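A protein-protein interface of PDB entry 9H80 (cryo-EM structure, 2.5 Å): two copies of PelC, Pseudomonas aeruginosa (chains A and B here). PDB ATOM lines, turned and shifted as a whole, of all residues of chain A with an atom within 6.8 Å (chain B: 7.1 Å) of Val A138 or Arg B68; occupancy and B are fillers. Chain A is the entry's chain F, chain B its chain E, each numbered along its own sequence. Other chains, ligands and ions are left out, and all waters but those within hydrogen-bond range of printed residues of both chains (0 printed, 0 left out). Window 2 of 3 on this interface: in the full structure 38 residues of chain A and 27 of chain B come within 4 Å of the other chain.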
ATOM      1  N   GLU A  25      14.500 -15.957  24.155  1.00  0.00           N
ATOM      2  CA  GLU A  25      13.320 -16.782  24.370  1.00  0.00           C
ATOM      3  C   GLU A  25      13.589 -17.801  25.469  1.00  0.00           C
ATOM      4  O   GLU A  25      14.667 -18.402  25.526  1.00  0.00           O
ATOM      5  CB  GLU A  25      12.924 -17.475  23.067  1.00  0.00           C
ATOM      6  CG  GLU A  25      11.724 -18.415  23.152  1.00  0.00           C
ATOM      7  CD  GLU A  25      10.410 -17.692  23.257  1.00  0.00           C
ATOM      8  OE1 GLU A  25      10.095 -16.892  22.355  1.00  0.00           O
ATOM      9  OE2 GLU A  25       9.680 -17.946  24.237  1.00  0.00           O
ATOM     10  N   SER A  26      12.602 -17.988  26.345  1.00  0.00           N
ATOM     11  CA  SER A  26      12.685 -18.914  27.467  1.00  0.00           C
ATOM     12  C   SER A  26      11.883 -20.185  27.216  1.00  0.00           C
ATOM     13  O   SER A  26      11.256 -20.716  28.139  1.00  0.00           O
ATOM     14  CB  SER A  26      12.205 -18.231  28.746  1.00  0.00           C
ATOM     15  OG  SER A  26      10.804 -18.027  28.714  1.00  0.00           O
ATOM     16  N   ALA A  27      11.894 -20.680  25.985  1.00  0.00           N
ATOM     17  CA  ALA A  27      11.079 -21.809  25.568  1.00  0.00           C
ATOM     18  C   ALA A  27      11.960 -23.014  25.260  1.00  0.00           C
ATOM     19  O   ALA A  27      13.189 -22.930  25.229  1.00  0.00           O
ATOM     20  CB  ALA A  27      10.236 -21.439  24.345  1.00  0.00           C
ATOM     21  N   LEU A 128      11.193 -12.499  15.015  1.00  0.00           N
ATOM     22  CA  LEU A 128      11.167 -13.857  14.488  1.00  0.00           C
ATOM     23  C   LEU A 128      10.277 -14.710  15.376  1.00  0.00           C
ATOM     24  O   LEU A 128      10.491 -14.772  16.590  1.00  0.00           O
ATOM     25  CB  LEU A 128      12.577 -14.448  14.422  1.00  0.00           C
ATOM     26  CG  LEU A 128      12.723 -15.746  13.626  1.00  0.00           C
ATOM     27  CD1 LEU A 128      12.866 -15.445  12.146  1.00  0.00           C
ATOM     28  CD2 LEU A 128      13.907 -16.550  14.128  1.00  0.00           C
ATOM     29  N   GLN A 129       9.291 -15.369  14.771  1.00  0.00           N
ATOM     30  CA  GLN A 129       8.342 -16.202  15.496  1.00  0.00           C
ATOM     31  C   GLN A 129       8.205 -17.551  14.811  1.00  0.00           C
ATOM     32  O   GLN A 129       8.286 -17.643  13.583  1.00  0.00           O
ATOM     33  CB  GLN A 129       6.965 -15.536  15.586  1.00  0.00           C
ATOM     34  CG  GLN A 129       6.933 -14.266  16.404  1.00  0.00           C
ATOM     35  CD  GLN A 129       5.773 -13.373  16.023  1.00  0.00           C
ATOM     36  OE1 GLN A 129       4.613 -13.784  16.087  1.00  0.00           O
ATOM     37  NE2 GLN A 129       6.076 -12.146  15.618  1.00  0.00           N
ATOM     38  N   VAL A 130       7.998 -18.592  15.611  1.00  0.00           N
ATOM     39  CA  VAL A 130       7.725 -19.939  15.122  1.00  0.00           C
ATOM     40  C   VAL A 130       6.354 -20.347  15.636  1.00  0.00           C
ATOM     41  O   VAL A 130       6.110 -20.326  16.848  1.00  0.00           O
ATOM     42  CB  VAL A 130       8.797 -20.947  15.564  1.00  0.00           C
ATOM     43  CG1 VAL A 130       8.486 -22.324  15.000  1.00  0.00           C
ATOM     44  CG2 VAL A 130      10.180 -20.484  15.125  1.00  0.00           C
ATOM     45  N   LEU A 131       5.468 -20.723  14.719  1.00  0.00           N
ATOM     46  CA  LEU A 131       4.093 -21.073  15.033  1.00  0.00           C
ATOM     47  C   LEU A 131       3.841 -22.549  14.758  1.00  0.00           C
ATOM     48  O   LEU A 131       4.416 -23.132  13.834  1.00  0.00           O
ATOM     49  CB  LEU A 131       3.112 -20.232  14.212  1.00  0.00           C
ATOM     50  CG  LEU A 131       2.717 -18.876  14.796  1.00  0.00           C
ATOM     51  CD1 LEU A 131       3.944 -18.021  15.055  1.00  0.00           C
ATOM     52  CD2 LEU A 131       1.755 -18.166  13.861  1.00  0.00           C
ATOM     53  N   GLU A 132       2.974 -23.147  15.570  1.00  0.00           N
ATOM     54  CA  GLU A 132       2.487 -24.494  15.306  1.00  0.00           C
ATOM     55  C   GLU A 132       1.325 -24.377  14.321  1.00  0.00           C
ATOM     56  O   GLU A 132       0.285 -23.813  14.683  1.00  0.00           O
ATOM     57  CB  GLU A 132       2.046 -25.177  16.599  1.00  0.00           C
ATOM     58  CG  GLU A 132       2.493 -26.625  16.724  1.00  0.00           C
ATOM     59  CD  GLU A 132       2.301 -27.174  18.125  1.00  0.00           C
ATOM     60  OE1 GLU A 132       3.003 -28.141  18.487  1.00  0.00           O
ATOM     61  OE2 GLU A 132       1.448 -26.639  18.864  1.00  0.00           O
ATOM     62  N   SER A 135      -2.449 -25.525  15.505  1.00  0.00           N
ATOM     63  CA  SER A 135      -3.101 -24.718  16.531  1.00  0.00           C
ATOM     64  C   SER A 135      -2.911 -23.225  16.287  1.00  0.00           C
ATOM     65  O   SER A 135      -3.740 -22.416  16.717  1.00  0.00           O
ATOM     66  CB  SER A 135      -2.557 -25.095  17.909  1.00  0.00           C
ATOM     67  OG  SER A 135      -1.157 -24.884  17.975  1.00  0.00           O
ATOM     68  N   GLY A 136      -1.838 -22.845  15.601  1.00  0.00           N
ATOM     69  CA  GLY A 136      -1.462 -21.451  15.497  1.00  0.00           C
ATOM     70  C   GLY A 136      -0.746 -20.906  16.710  1.00  0.00           C
ATOM     71  O   GLY A 136      -0.464 -19.704  16.756  1.00  0.00           O
ATOM     72  N   ARG A 137      -0.445 -21.752  17.692  1.00  0.00           N
ATOM     73  CA  ARG A 137       0.222 -21.320  18.910  1.00  0.00           C
ATOM     74  C   ARG A 137       1.653 -20.900  18.609  1.00  0.00           C
ATOM     75  O   ARG A 137       2.342 -21.540  17.809  1.00  0.00           O
ATOM     76  CB  ARG A 137       0.206 -22.450  19.938  1.00  0.00           C
ATOM     77  CG  ARG A 137       1.048 -22.193  21.178  1.00  0.00           C
ATOM     78  CD  ARG A 137       0.618 -23.093  22.326  1.00  0.00           C
ATOM     79  NE  ARG A 137       0.880 -24.501  22.047  1.00  0.00           N
ATOM     80  CZ  ARG A 137       2.064 -25.089  22.155  1.00  0.00           C
ATOM     81  NH1 ARG A 137       3.137 -24.426  22.562  1.00  0.00           N
ATOM     82  NH2 ARG A 137       2.178 -26.380  21.853  1.00  0.00           N
ATOM     83  N   VAL A 138       2.098 -19.823  19.252  1.00  0.00           N
ATOM     84  CA  VAL A 138       3.471 -19.360  19.088  1.00  0.00           C
ATOM     85  C   VAL A 138       4.381 -20.209  19.964  1.00  0.00           C
ATOM     86  O   VAL A 138       4.216 -20.260  21.189  1.00  0.00           O
ATOM     87  CB  VAL A 138       3.592 -17.871  19.437  1.00  0.00           C
ATOM     88  CG1 VAL A 138       5.037 -17.410  19.325  1.00  0.00           C
ATOM     89  CG2 VAL A 138       2.689 -17.041  18.536  1.00  0.00           C
ATOM     90  N   LEU A 139       5.348 -20.880  19.338  1.00  0.00           N
ATOM     91  CA  LEU A 139       6.310 -21.710  20.049  1.00  0.00           C
ATOM     92  C   LEU A 139       7.626 -20.997  20.318  1.00  0.00           C
ATOM     93  O   LEU A 139       8.360 -21.401  21.225  1.00  0.00           O
ATOM     94  CB  LEU A 139       6.602 -22.990  19.255  1.00  0.00           C
ATOM     95  CG  LEU A 139       5.415 -23.718  18.620  1.00  0.00           C
ATOM     96  CD1 LEU A 139       5.898 -24.765  17.636  1.00  0.00           C
ATOM     97  CD2 LEU A 139       4.547 -24.345  19.691  1.00  0.00           C
ATOM     98  N   TRP A 140       7.938 -19.955  19.550  1.00  0.00           N
ATOM     99  CA  TRP A 140       9.177 -19.211  19.697  1.00  0.00           C
ATOM    100  C   TRP A 140       8.890 -17.772  19.301  1.00  0.00           C
ATOM    101  O   TRP A 140       8.067 -17.528  18.417  1.00  0.00           O
ATOM    102  CB  TRP A 140      10.285 -19.808  18.822  1.00  0.00           C
ATOM    103  CG  TRP A 140      11.656 -19.312  19.131  1.00  0.00           C
ATOM    104  CD1 TRP A 140      12.250 -18.187  18.645  1.00  0.00           C
ATOM    105  CD2 TRP A 140      12.616 -19.939  19.983  1.00  0.00           C
ATOM    106  NE1 TRP A 140      13.522 -18.068  19.151  1.00  0.00           N
ATOM    107  CE2 TRP A 140      13.768 -19.132  19.978  1.00  0.00           C
ATOM    108  CE3 TRP A 140      12.611 -21.101  20.759  1.00  0.00           C
ATOM    109  CZ2 TRP A 140      14.905 -19.452  20.713  1.00  0.00           C
ATOM    110  CZ3 TRP A 140      13.738 -21.415  21.490  1.00  0.00           C
ATOM    111  CH2 TRP A 140      14.869 -20.594  21.463  1.00  0.00           C
ATOM    112  N   SER A 141       9.544 -16.826  19.970  1.00  0.00           N
ATOM    113  CA  SER A 141       9.320 -15.414  19.671  1.00  0.00           C
ATOM    114  C   SER A 141      10.523 -14.620  20.162  1.00  0.00           C
ATOM    115  O   SER A 141      10.705 -14.464  21.372  1.00  0.00           O
ATOM    116  CB  SER A 141       8.034 -14.922  20.320  1.00  0.00           C
ATOM    117  OG  SER A 141       7.664 -13.655  19.812  1.00  0.00           O
ATOM    118  N   ARG B  32       2.155 -15.615  37.204  1.00  0.00           N
ATOM    119  CA  ARG B  32       2.704 -15.994  35.907  1.00  0.00           C
ATOM    120  C   ARG B  32       1.898 -17.123  35.278  1.00  0.00           C
ATOM    121  O   ARG B  32       1.608 -17.093  34.077  1.00  0.00           O
ATOM    122  CB  ARG B  32       4.170 -16.402  36.060  1.00  0.00           C
ATOM    123  CG  ARG B  32       4.859 -16.787  34.753  1.00  0.00           C
ATOM    124  CD  ARG B  32       6.311 -17.172  34.980  1.00  0.00           C
ATOM    125  NE  ARG B  32       7.183 -16.003  35.066  1.00  0.00           N
ATOM    126  CZ  ARG B  32       7.837 -15.593  36.149  1.00  0.00           C
ATOM    127  NH1 ARG B  32       7.729 -16.215  37.314  1.00  0.00           N
ATOM    128  NH2 ARG B  32       8.620 -14.523  36.062  1.00  0.00           N
ATOM    129  N   ALA B  34      -1.060 -18.140  34.443  1.00  0.00           N
ATOM    130  CA  ALA B  34      -2.441 -17.740  34.226  1.00  0.00           C
ATOM    131  C   ALA B  34      -2.696 -17.637  32.730  1.00  0.00           C
ATOM    132  O   ALA B  34      -1.771 -17.686  31.915  1.00  0.00           O
ATOM    133  CB  ALA B  34      -2.749 -16.411  34.925  1.00  0.00           C
ATOM    134  N   GLN B  35      -3.970 -17.504  32.369  1.00  0.00           N
ATOM    135  CA  GLN B  35      -4.374 -17.374  30.970  1.00  0.00           C
ATOM    136  C   GLN B  35      -4.242 -15.911  30.563  1.00  0.00           C
ATOM    137  O   GLN B  35      -5.138 -15.096  30.781  1.00  0.00           O
ATOM    138  CB  GLN B  35      -5.797 -17.883  30.771  1.00  0.00           C
ATOM    139  CG  GLN B  35      -5.946 -19.385  30.928  1.00  0.00           C
ATOM    140  CD  GLN B  35      -5.547 -20.144  29.679  1.00  0.00           C
ATOM    141  OE1 GLN B  35      -4.445 -19.972  29.160  1.00  0.00           O
ATOM    142  NE2 GLN B  35      -6.445 -20.992  29.189  1.00  0.00           N
ATOM    143  N   TRP B  36      -3.103 -15.580  29.962  1.00  0.00           N
ATOM    144  CA  TRP B  36      -2.836 -14.217  29.526  1.00  0.00           C
ATOM    145  C   TRP B  36      -3.383 -13.974  28.126  1.00  0.00           C
ATOM    146  O   TRP B  36      -3.396 -14.875  27.284  1.00  0.00           O
ATOM    147  CB  TRP B  36      -1.333 -13.938  29.533  1.00  0.00           C
ATOM    148  CG  TRP B  36      -0.728 -13.817  30.891  1.00  0.00           C
ATOM    149  CD1 TRP B  36      -0.448 -14.828  31.755  1.00  0.00           C
ATOM    150  CD2 TRP B  36      -0.307 -12.610  31.531  1.00  0.00           C
ATOM    151  NE1 TRP B  36       0.119 -14.327  32.901  1.00  0.00           N
ATOM    152  CE2 TRP B  36       0.217 -12.967  32.787  1.00  0.00           C
ATOM    153  CE3 TRP B  36      -0.323 -11.263  31.165  1.00  0.00           C
ATOM    154  CZ2 TRP B  36       0.715 -12.024  33.680  1.00  0.00           C
ATOM    155  CZ3 TRP B  36       0.173 -10.330  32.051  1.00  0.00           C
ATOM    156  CH2 TRP B  36       0.685 -10.713  33.294  1.00  0.00           C
ATOM    157  N   GLY B  37      -3.837 -12.744  27.888  1.00  0.00           N
ATOM    158  CA  GLY B  37      -4.208 -12.280  26.570  1.00  0.00           C
ATOM    159  C   GLY B  37      -3.362 -11.080  26.172  1.00  0.00           C
ATOM    160  O   GLY B  37      -2.496 -10.621  26.912  1.00  0.00           O
ATOM    161  N   LEU B  59       5.442  -8.839  22.542  1.00  0.00           N
ATOM    162  CA  LEU B  59       5.277 -10.286  22.510  1.00  0.00           C
ATOM    163  C   LEU B  59       6.624 -10.974  22.661  1.00  0.00           C
ATOM    164  O   LEU B  59       6.739 -11.984  23.366  1.00  0.00           O
ATOM    165  CB  LEU B  59       4.596 -10.707  21.207  1.00  0.00           C
ATOM    166  CG  LEU B  59       4.325 -12.203  21.007  1.00  0.00           C
ATOM    167  CD1 LEU B  59       3.310 -12.705  22.020  1.00  0.00           C
ATOM    168  CD2 LEU B  59       3.855 -12.481  19.590  1.00  0.00           C
ATOM    169  N   LEU B  62       7.751 -10.371  26.482  1.00  0.00           N
ATOM    170  CA  LEU B  62       7.032 -11.199  27.441  1.00  0.00           C
ATOM    171  C   LEU B  62       7.465 -12.654  27.352  1.00  0.00           C
ATOM    172  O   LEU B  62       7.537 -13.342  28.375  1.00  0.00           O
ATOM    173  CB  LEU B  62       5.527 -11.084  27.206  1.00  0.00           C
ATOM    174  CG  LEU B  62       4.863  -9.794  27.683  1.00  0.00           C
ATOM    175  CD1 LEU B  62       3.548  -9.574  26.958  1.00  0.00           C
ATOM    176  CD2 LEU B  62       4.640  -9.837  29.181  1.00  0.00           C
ATOM    177  N   ALA B  63       7.748 -13.138  26.142  1.00  0.00           N
ATOM    178  CA  ALA B  63       8.256 -14.495  25.986  1.00  0.00           C
ATOM    179  C   ALA B  63       9.575 -14.680  26.723  1.00  0.00           C
ATOM    180  O   ALA B  63       9.828 -15.753  27.279  1.00  0.00           O
ATOM    181  CB  ALA B  63       8.423 -14.815  24.502  1.00  0.00           C
ATOM    182  N   GLU B  64      10.421 -13.648  26.734  1.00  0.00           N
ATOM    183  CA  GLU B  64      11.636 -13.680  27.540  1.00  0.00           C
ATOM    184  C   GLU B  64      11.329 -13.910  29.012  1.00  0.00           C
ATOM    185  O   GLU B  64      12.130 -14.526  29.723  1.00  0.00           O
ATOM    186  CB  GLU B  64      12.401 -12.369  27.361  1.00  0.00           C
ATOM    187  CG  GLU B  64      13.845 -12.399  27.820  1.00  0.00           C
ATOM    188  CD  GLU B  64      14.557 -11.085  27.585  1.00  0.00           C
ATOM    189  OE1 GLU B  64      14.044 -10.260  26.802  1.00  0.00           O
ATOM    190  OE2 GLU B  64      15.635 -10.878  28.179  1.00  0.00           O
ATOM    191  N   GLU B  65      10.181 -13.428  29.483  1.00  0.00           N
ATOM    192  CA  GLU B  65       9.795 -13.515  30.884  1.00  0.00           C
ATOM    193  C   GLU B  65       8.901 -14.715  31.182  1.00  0.00           C
ATOM    194  O   GLU B  65       8.314 -14.778  32.266  1.00  0.00           O
ATOM    195  CB  GLU B  65       9.084 -12.225  31.305  1.00  0.00           C
ATOM    196  CG  GLU B  65       9.606 -11.608  32.593  1.00  0.00           C
ATOM    197  CD  GLU B  65      11.043 -11.132  32.480  1.00  0.00           C
ATOM    198  OE1 GLU B  65      11.272 -10.062  31.877  1.00  0.00           O
ATOM    199  OE2 GLU B  65      11.943 -11.827  32.996  1.00  0.00           O
ATOM    200  N   GLY B  66       8.781 -15.659  30.254  1.00  0.00           N
ATOM    201  CA  GLY B  66       7.989 -16.846  30.499  1.00  0.00           C
ATOM    202  C   GLY B  66       6.497 -16.665  30.355  1.00  0.00           C
ATOM    203  O   GLY B  66       5.736 -17.509  30.839  1.00  0.00           O
ATOM    204  N   VAL B  67       6.053 -15.594  29.703  1.00  0.00           N
ATOM    205  CA  VAL B  67       4.636 -15.300  29.518  1.00  0.00           C
ATOM    206  C   VAL B  67       4.325 -15.468  28.038  1.00  0.00           C
ATOM    207  O   VAL B  67       4.941 -14.809  27.190  1.00  0.00           O
ATOM    208  CB  VAL B  67       4.272 -13.890  30.001  1.00  0.00           C
ATOM    209  CG1 VAL B  67       2.791 -13.608  29.763  1.00  0.00           C
ATOM    210  CG2 VAL B  67       4.622 -13.724  31.472  1.00  0.00           C
ATOM    211  N   ARG B  68       3.370 -16.344  27.727  1.00  0.00           N
ATOM    212  CA  ARG B  68       2.911 -16.572  26.359  1.00  0.00           C
ATOM    213  C   ARG B  68       1.434 -16.206  26.269  1.00  0.00           C
ATOM    214  O   ARG B  68       0.569 -17.058  26.526  1.00  0.00           O
ATOM    215  CB  ARG B  68       3.132 -18.032  25.951  1.00  0.00           C
ATOM    216  CG  ARG B  68       4.481 -18.587  26.356  1.00  0.00           C
ATOM    217  CD  ARG B  68       4.926 -19.691  25.409  1.00  0.00           C
ATOM    218  NE  ARG B  68       5.457 -19.160  24.157  1.00  0.00           N
ATOM    219  CZ  ARG B  68       6.608 -18.513  24.038  1.00  0.00           C
ATOM    220  NH1 ARG B  68       7.403 -18.309  25.077  1.00  0.00           N
ATOM    221  NH2 ARG B  68       6.976 -18.057  22.843  1.00  0.00           N
ATOM    222  N   PRO B  69       1.086 -14.967  25.923  1.00  0.00           N
ATOM    223  CA  PRO B  69      -0.328 -14.584  25.900  1.00  0.00           C
ATOM    224  C   PRO B  69      -1.020 -14.987  24.608  1.00  0.00           C
ATOM    225  O   PRO B  69      -0.409 -15.036  23.538  1.00  0.00           O
ATOM    226  CB  PRO B  69      -0.279 -13.061  26.046  1.00  0.00           C
ATOM    227  CG  PRO B  69       1.014 -12.670  25.454  1.00  0.00           C
ATOM    228  CD  PRO B  69       1.966 -13.818  25.645  1.00  0.00           C
ATOM    229  N   ARG B  70      -2.313 -15.274  24.721  1.00  0.00           N
ATOM    230  CA  ARG B  70      -3.134 -15.540  23.547  1.00  0.00           C
ATOM    231  C   ARG B  70      -3.376 -14.235  22.802  1.00  0.00           C
ATOM    232  O   ARG B  70      -3.907 -13.278  23.371  1.00  0.00           O
ATOM    233  CB  ARG B  70      -4.462 -16.171  23.955  1.00  0.00           C
ATOM    234  CG  ARG B  70      -4.341 -17.412  24.832  1.00  0.00           C
ATOM    235  CD  ARG B  70      -4.916 -18.647  24.151  1.00  0.00           C
ATOM    236  NE  ARG B  70      -6.371 -18.687  24.230  1.00  0.00           N
ATOM    237  CZ  ARG B  70      -7.064 -18.925  25.336  1.00  0.00           C
ATOM    238  NH1 ARG B  70      -6.468 -19.162  26.494  1.00  0.00           N
ATOM    239  NH2 ARG B  70      -8.393 -18.925  25.279  1.00  0.00           N
ATOM    240  N   LEU B  71      -2.987 -14.192  21.533  1.00  0.00           N
ATOM    241  CA  LEU B  71      -3.148 -12.983  20.743  1.00  0.00           C
ATOM    242  C   LEU B  71      -4.592 -12.848  20.280  1.00  0.00           C
ATOM    243  O   LEU B  71      -5.271 -13.838  19.998  1.00  0.00           O
ATOM    244  CB  LEU B  71      -2.212 -12.991  19.531  1.00  0.00           C
ATOM    245  CG  LEU B  71      -0.836 -13.644  19.692  1.00  0.00           C
ATOM    246  CD1 LEU B  71      -0.073 -13.599  18.382  1.00  0.00           C
ATOM    247  CD2 LEU B  71      -0.041 -12.977  20.802  1.00  0.00           C
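The backbone carbonyl oxygen (O) of Ala B63 lies within hydrogen-bond range of the side-chain hydroxyl (OG) of Ser A26 (2.9 Å).
The side-chain hydroxyl of Ser A26 sits at hydrogen-bond distance from the backbone NH of Gly B66.
The guanidinium group of Arg B68 is in salt-bridge range of the side-chain carboxylate of Glu A25 (2.5 Å).
The backbone carbonyl oxygen (O) of Val A138 is in hydrogen-bond range of the guanidinium group (NE) of Arg B68, at 3.4 Å.
The side-chain carboxylate (OE1) of Glu A25 is in hydrogen-bond range of the backbone NH (N) of Ser A141 (2.4 Å).
The backbone NH (N) of Leu A139 is in hydrogen-bond range of the backbone carbonyl oxygen (O) of Val A130, at 2.7 Å.
The backbone carbonyl oxygen (O) of Trp A140 sits at hydrogen-bond distance from the backbone NH (N) of Val A130 (3.0 Å).
Among the printed residues, merely in contact across the chains: Glu A25 with Ala B63, Gln A129 with Leu B59, Ser A141 with Leu B59, Ser A26 with Glu B64, Ser A141 with Ala B63, Trp A140 with Arg B68 and Leu A139 with Arg B68.
Val A138 touches just one residue of chain B: Arg B68 (3.4 Å).
Of the printed residues of chain B, Trp A140 touches Arg B68 (3.9 Å).
Printed residues of chain B within 4 Å of Ser A141: Leu B59 (3.8 Å) and Ala B63 (3.9 Å).
Of the printed residues of chain A, Leu B59 touches Gln A129 (3.8 Å) and Ser A141 (3.8 Å).
Of chain A, only Glu A25, Val A138, Leu A139 and Trp A140 come within 4 Å of Arg B68.
The nearest residue of chain A that does not touch Arg B68 is Ser A141 (4.05 Å).
Hydrophobic or aromatic side chains of chain B that line the printed part of chain A: Leu B59 and Ala B63.
Among the printed residues, 11 pairs touch across the chains.
Among the printed residues, Asp or Glu carboxylates within 4 Å of a Lys or Arg side-chain nitrogen of the other chain: Glu A25 with Arg B68 (2.5 Å).
No position is printed for both chains.
Of the 11 pairs that touch across the chains among the printed residues, none has its exchanged pair printed and touching as well.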
